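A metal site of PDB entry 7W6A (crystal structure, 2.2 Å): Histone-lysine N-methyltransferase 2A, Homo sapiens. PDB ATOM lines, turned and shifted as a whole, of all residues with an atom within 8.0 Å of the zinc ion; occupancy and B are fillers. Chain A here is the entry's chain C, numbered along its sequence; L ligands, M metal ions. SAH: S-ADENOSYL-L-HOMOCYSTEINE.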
ATOM      1  N   ILE A  27       3.889  15.543  22.716  1.00  0.00           N
ATOM      2  CA  ILE A  27       3.796  17.006  22.775  1.00  0.00           C
ATOM      3  C   ILE A  27       4.811  17.572  21.800  1.00  0.00           C
ATOM      4  O   ILE A  27       4.469  18.354  20.901  1.00  0.00           O
ATOM      5  CB  ILE A  27       4.042  17.545  24.185  1.00  0.00           C
ATOM      6  CG1 ILE A  27       2.900  17.186  25.148  1.00  0.00           C
ATOM      7  CG2 ILE A  27       4.220  19.059  24.140  1.00  0.00           C
ATOM      8  CD1 ILE A  27       3.106  17.693  26.555  1.00  0.00           C
ATOM      9  N   HIS A  97       6.606  21.808  27.907  1.00  0.00           N
ATOM     10  CA  HIS A  97       5.653  22.741  28.513  1.00  0.00           C
ATOM     11  C   HIS A  97       4.236  22.199  28.385  1.00  0.00           C
ATOM     12  O   HIS A  97       3.877  21.537  27.405  1.00  0.00           O
ATOM     13  CB  HIS A  97       5.729  24.115  27.833  1.00  0.00           C
ATOM     14  CG  HIS A  97       4.520  24.969  28.071  1.00  0.00           C
ATOM     15  ND1 HIS A  97       4.428  25.832  29.137  1.00  0.00           N
ATOM     16  CD2 HIS A  97       3.350  25.053  27.412  1.00  0.00           C
ATOM     17  CE1 HIS A  97       3.249  26.440  29.114  1.00  0.00           C
ATOM     18  NE2 HIS A  97       2.571  25.974  28.069  1.00  0.00           N
ATOM     19  N   SER A  98       3.409  22.487  29.391  1.00  0.00           N
ATOM     20  CA  SER A  98       1.996  22.182  29.317  1.00  0.00           C
ATOM     21  C   SER A  98       1.197  23.342  29.894  1.00  0.00           C
ATOM     22  O   SER A  98       1.587  23.919  30.907  1.00  0.00           O
ATOM     23  CB  SER A  98       1.618  20.907  30.066  1.00  0.00           C
ATOM     24  OG  SER A  98       0.209  20.720  30.046  1.00  0.00           O
ATOM     25  N   CYS A  99       0.081  23.664  29.247  1.00  0.00           N
ATOM     26  CA  CYS A  99      -0.817  24.682  29.777  1.00  0.00           C
ATOM     27  C   CYS A  99      -1.586  24.176  30.991  1.00  0.00           C
ATOM     28  O   CYS A  99      -2.114  24.987  31.758  1.00  0.00           O
ATOM     29  CB  CYS A  99      -1.758  25.182  28.681  1.00  0.00           C
ATOM     30  SG  CYS A  99      -0.888  25.817  27.208  1.00  0.00           S
ATOM     31  N   GLU A 100      -1.647  22.857  31.190  1.00  0.00           N
ATOM     32  CA  GLU A 100      -2.161  22.279  32.421  1.00  0.00           C
ATOM     33  C   GLU A 100      -1.134  21.261  32.908  1.00  0.00           C
ATOM     34  O   GLU A 100      -1.314  20.040  32.769  1.00  0.00           O
ATOM     35  CB  GLU A 100      -3.555  21.683  32.215  1.00  0.00           C
ATOM     36  CG  GLU A 100      -4.684  22.660  32.612  1.00  0.00           C
ATOM     37  CD  GLU A 100      -6.083  22.193  32.241  1.00  0.00           C
ATOM     38  OE1 GLU A 100      -6.230  21.317  31.350  1.00  0.00           O
ATOM     39  OE2 GLU A 100      -7.061  22.715  32.842  1.00  0.00           O
ATOM     40  N   PRO A 146       3.703  28.118  18.483  1.00  0.00           N
ATOM     41  CA  PRO A 146       2.476  27.407  18.850  1.00  0.00           C
ATOM     42  C   PRO A 146       2.744  26.327  19.881  1.00  0.00           C
ATOM     43  O   PRO A 146       3.833  25.750  19.943  1.00  0.00           O
ATOM     44  CB  PRO A 146       1.990  26.815  17.515  1.00  0.00           C
ATOM     45  CG  PRO A 146       2.782  27.520  16.451  1.00  0.00           C
ATOM     46  CD  PRO A 146       4.088  27.861  17.085  1.00  0.00           C
ATOM     47  N   CYS A 147       1.728  26.045  20.677  1.00  0.00           N
ATOM     48  CA  CYS A 147       1.794  25.020  21.710  1.00  0.00           C
ATOM     49  C   CYS A 147       1.133  23.734  21.233  1.00  0.00           C
ATOM     50  O   CYS A 147       0.091  23.762  20.559  1.00  0.00           O
ATOM     51  CB  CYS A 147       1.127  25.505  22.990  1.00  0.00           C
ATOM     52  SG  CYS A 147       1.151  24.262  24.310  1.00  0.00           S
ATOM     53  N   ASN A 148       1.744  22.589  21.584  1.00  0.00           N
ATOM     54  CA  ASN A 148       1.249  21.272  21.214  1.00  0.00           C
ATOM     55  C   ASN A 148       0.989  20.411  22.450  1.00  0.00           C
ATOM     56  O   ASN A 148       1.044  19.182  22.378  1.00  0.00           O
ATOM     57  CB  ASN A 148       2.232  20.582  20.274  1.00  0.00           C
ATOM     58  CG  ASN A 148       1.589  19.468  19.448  1.00  0.00           C
ATOM     59  OD1 ASN A 148       0.545  19.672  18.838  1.00  0.00           O
ATOM     60  ND2 ASN A 148       2.219  18.295  19.434  1.00  0.00           N
ATOM     61  N   CYS A 149       0.702  21.056  23.591  1.00  0.00           N
ATOM     62  CA  CYS A 149       0.570  20.317  24.852  1.00  0.00           C
ATOM     63  C   CYS A 149      -0.669  19.425  24.873  1.00  0.00           C
ATOM     64  O   CYS A 149      -0.711  18.468  25.655  1.00  0.00           O
ATOM     65  CB  CYS A 149       0.549  21.288  26.038  1.00  0.00           C
ATOM     66  SG  CYS A 149      -1.035  22.111  26.388  1.00  0.00           S
ATOM     67  N   GLY A 150      -1.668  19.714  24.050  1.00  0.00           N
ATOM     68  CA  GLY A 150      -2.794  18.829  23.887  1.00  0.00           C
ATOM     69  C   GLY A 150      -3.838  18.885  24.985  1.00  0.00           C
ATOM     70  O   GLY A 150      -4.734  18.025  25.001  1.00  0.00           O
ATOM     71  N   ALA A 151      -3.751  19.845  25.888  1.00  0.00           N
ATOM     72  CA  ALA A 151      -4.778  20.037  26.899  1.00  0.00           C
ATOM     73  C   ALA A 151      -5.950  20.826  26.332  1.00  0.00           C
ATOM     74  O   ALA A 151      -5.832  21.492  25.288  1.00  0.00           O
ATOM     75  CB  ALA A 151      -4.209  20.761  28.117  1.00  0.00           C
ATOM     76  N   LYS A 152      -7.099  20.762  27.004  1.00  0.00           N
ATOM     77  CA  LYS A 152      -8.258  21.493  26.511  1.00  0.00           C
ATOM     78  C   LYS A 152      -8.314  22.931  26.998  1.00  0.00           C
ATOM     79  O   LYS A 152      -9.006  23.739  26.385  1.00  0.00           O
ATOM     80  CB  LYS A 152      -9.553  20.764  26.877  1.00  0.00           C
ATOM     81  CG  LYS A 152      -9.674  20.358  28.325  1.00  0.00           C
ATOM     82  CD  LYS A 152     -11.048  19.724  28.540  1.00  0.00           C
ATOM     83  CE  LYS A 152     -11.236  18.539  27.599  1.00  0.00           C
ATOM     84  NZ  LYS A 152     -12.586  17.934  27.728  1.00  0.00           N
ATOM     85  N   LYS A 153      -7.589  23.273  28.065  1.00  0.00           N
ATOM     86  CA  LYS A 153      -7.368  24.668  28.429  1.00  0.00           C
ATOM     87  C   LYS A 153      -6.081  25.216  27.825  1.00  0.00           C
ATOM     88  O   LYS A 153      -5.471  26.125  28.405  1.00  0.00           O
ATOM     89  CB  LYS A 153      -7.368  24.832  29.946  1.00  0.00           C
ATOM     90  CG  LYS A 153      -8.708  24.574  30.621  1.00  0.00           C
ATOM     91  CD  LYS A 153      -9.039  25.635  31.664  1.00  0.00           C
ATOM     92  CE  LYS A 153     -10.484  25.491  32.148  1.00  0.00           C
ATOM     93  NZ  LYS A 153     -11.479  25.933  31.117  1.00  0.00           N
ATOM     94  N   CYS A 154      -5.657  24.671  26.685  1.00  0.00           N
ATOM     95  CA  CYS A 154      -4.424  25.122  26.045  1.00  0.00           C
ATOM     96  C   CYS A 154      -4.549  26.571  25.606  1.00  0.00           C
ATOM     97  O   CYS A 154      -5.613  27.016  25.163  1.00  0.00           O
ATOM     98  CB  CYS A 154      -4.114  24.227  24.849  1.00  0.00           C
ATOM     99  SG  CYS A 154      -2.576  24.628  23.966  1.00  0.00           S
ATOM    100  N   ARG A 155      -3.451  27.291  25.730  1.00  0.00           N
ATOM    101  CA  ARG A 155      -3.404  28.742  25.398  1.00  0.00           C
ATOM    102  C   ARG A 155      -3.007  28.944  23.936  1.00  0.00           C
ATOM    103  O   ARG A 155      -2.705  30.066  23.604  1.00  0.00           O
ATOM    104  CB  ARG A 155      -2.438  29.457  26.329  1.00  0.00           C
ATOM    105  CG  ARG A 155      -2.701  29.164  27.796  1.00  0.00           C
ATOM    106  CD  ARG A 155      -2.050  30.089  28.802  1.00  0.00           C
ATOM    107  NE  ARG A 155      -0.614  30.003  28.843  1.00  0.00           N
ATOM    108  CZ  ARG A 155       0.088  29.542  29.870  1.00  0.00           C
ATOM    109  NH1 ARG A 155       1.404  29.524  29.796  1.00  0.00           N
ATOM    110  NH2 ARG A 155      -0.519  29.125  30.951  1.00  0.00           N
ATOM    111  N   LYS A 156      -2.809  27.880  23.164  1.00  0.00           N
ATOM    112  CA  LYS A 156      -2.448  27.887  21.723  1.00  0.00           C
ATOM    113  C   LYS A 156      -0.968  28.196  21.439  1.00  0.00           C
ATOM    114  O   LYS A 156      -0.459  27.666  20.483  1.00  0.00           O
ATOM    115  CB  LYS A 156      -3.450  28.627  20.843  1.00  0.00           C
ATOM    116  N   PHE A 157      -0.329  29.072  22.211  1.00  0.00           N
ATOM    117  CA  PHE A 157       1.094  29.459  22.034  1.00  0.00           C
ATOM    118  C   PHE A 157       1.794  29.451  23.382  1.00  0.00           C
ATOM    119  O   PHE A 157       1.167  29.692  24.407  1.00  0.00           O
ATOM    120  CB  PHE A 157       1.174  30.878  21.467  1.00  0.00           C
ATOM    121  CG  PHE A 157       0.314  31.099  20.251  1.00  0.00           C
ATOM    122  CD1 PHE A 157       0.539  30.410  19.072  1.00  0.00           C
ATOM    123  CD2 PHE A 157      -0.754  31.966  20.297  1.00  0.00           C
ATOM    124  CE1 PHE A 157      -0.268  30.599  17.973  1.00  0.00           C
ATOM    125  CE2 PHE A 157      -1.556  32.151  19.190  1.00  0.00           C
ATOM    126  CZ  PHE A 157      -1.311  31.480  18.031  1.00  0.00           C
ATOM    127  N   LEU A 158       3.091  29.178  23.341  1.00  0.00           N
ATOM    128  CA  LEU A 158       4.008  29.183  24.511  1.00  0.00           C
ATOM    129  C   LEU A 158       4.114  30.598  25.071  1.00  0.00           C
ATOM    130  O   LEU A 158       4.326  30.727  26.259  1.00  0.00           O
ATOM    131  CB  LEU A 158       5.390  28.754  24.039  1.00  0.00           C
ATOM    132  CG  LEU A 158       5.566  27.269  23.775  1.00  0.00           C
ATOM    133  CD1 LEU A 158       5.588  26.501  25.067  1.00  0.00           C
ATOM    134  CD2 LEU A 158       4.466  26.749  22.884  1.00  0.00           C
HETATM  135  N   SAH L   1      10.835  18.729  23.638  1.00  0.00           N
HETATM  136  CA  SAH L   1      12.225  19.164  23.574  1.00  0.00           C
HETATM  137  CB  SAH L   1      12.790  19.379  24.975  1.00  0.00           C
HETATM  138  CG  SAH L   1      12.335  20.666  25.649  1.00  0.00           C
HETATM  139  SD  SAH L   1      13.494  22.028  25.364  1.00  0.00           S
HETATM  140  C   SAH L   1      13.089  18.151  22.809  1.00  0.00           C
HETATM  141  O   SAH L   1      12.628  17.115  22.338  1.00  0.00           O
HETATM  142  OXT SAH L   1      14.283  18.374  22.646  1.00  0.00           O
HETATM  143  C5' SAH L   1      12.147  23.177  25.023  1.00  0.00           C
HETATM  144  C4' SAH L   1      11.763  23.163  23.558  1.00  0.00           C
HETATM  145  O4' SAH L   1      10.814  22.136  23.309  1.00  0.00           O
HETATM  146  C3' SAH L   1      11.126  24.477  23.139  1.00  0.00           C
HETATM  147  O3' SAH L   1      12.073  25.236  22.422  1.00  0.00           O
HETATM  148  C2' SAH L   1       9.982  24.076  22.244  1.00  0.00           C
HETATM  149  O2' SAH L   1      10.386  24.219  20.904  1.00  0.00           O
HETATM  150  C1' SAH L   1       9.729  22.608  22.528  1.00  0.00           C
HETATM  151  N9  SAH L   1       8.469  22.502  23.296  1.00  0.00           N
HETATM  152  C8  SAH L   1       8.338  22.418  24.660  1.00  0.00           C
HETATM  153  N7  SAH L   1       7.026  22.352  24.982  1.00  0.00           N
HETATM  154  C5  SAH L   1       6.301  22.408  23.831  1.00  0.00           C
HETATM  155  C6  SAH L   1       4.936  22.393  23.572  1.00  0.00           C
HETATM  156  N6  SAH L   1       4.050  22.308  24.557  1.00  0.00           N
HETATM  157  N1  SAH L   1       4.497  22.457  22.267  1.00  0.00           N
HETATM  158  C2  SAH L   1       5.403  22.551  21.228  1.00  0.00           C
HETATM  159  N3  SAH L   1       6.754  22.567  21.489  1.00  0.00           N
HETATM  160  C4  SAH L   1       7.202  22.501  22.762  1.00  0.00           C
HETATM  161 ZN    ZN M   1      -0.822  24.286  25.491  1.00  0.00          ZN
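The backbone NH (N) of His 97 lies within hydrogen-bond range of a nitrogen (N7) of the ligand, at 3.0 Å.
N of Asn 148 lies within hydrogen-bond range of N1 of the ligand (2.8 Å).
The backbone carbonyl oxygen (O) of His 97 sits at hydrogen-bond distance from a nitrogen (N6) of the ligand, 3.0 Å away.
The side-chain sulfur (SG) of Cys 147 sits close to a nitrogen (N6) of the ligand, 3.5 Å away.
The side-chain sulfur (SG) of Cys 154 lies close to the backbone NH (N) of Lys 156 (3.4 Å).
O of Lys 156 lies within hydrogen-bond range of N of Cys 147, 2.7 Å away.
The backbone NH of Arg 155 sits close to the side-chain sulfur of Cys 99 (3.3 Å).
The side-chain sulfur of Cys 149 sits close to the backbone NH of Ala 151 (3.6 Å).
The side-chain sulfur (SG) of Cys 99 sits close to a ring nitrogen (NE2) of His 97 (3.6 Å).
N of Arg 155 touches the zinc ion, at 3.9998 Å.
Of the 18 residues printed, 5 come within 4 Å of the zinc ion.
The nearest printed residue that does not touch the zinc ion is His 97 (4.6 Å).
The zinc ion is bound by SG of Cys 147 (2.3 Å), SG of Cys 99 (2.3 Å), SG of Cys 154 (2.3 Å) and SG of Cys 149 (2.4 Å).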
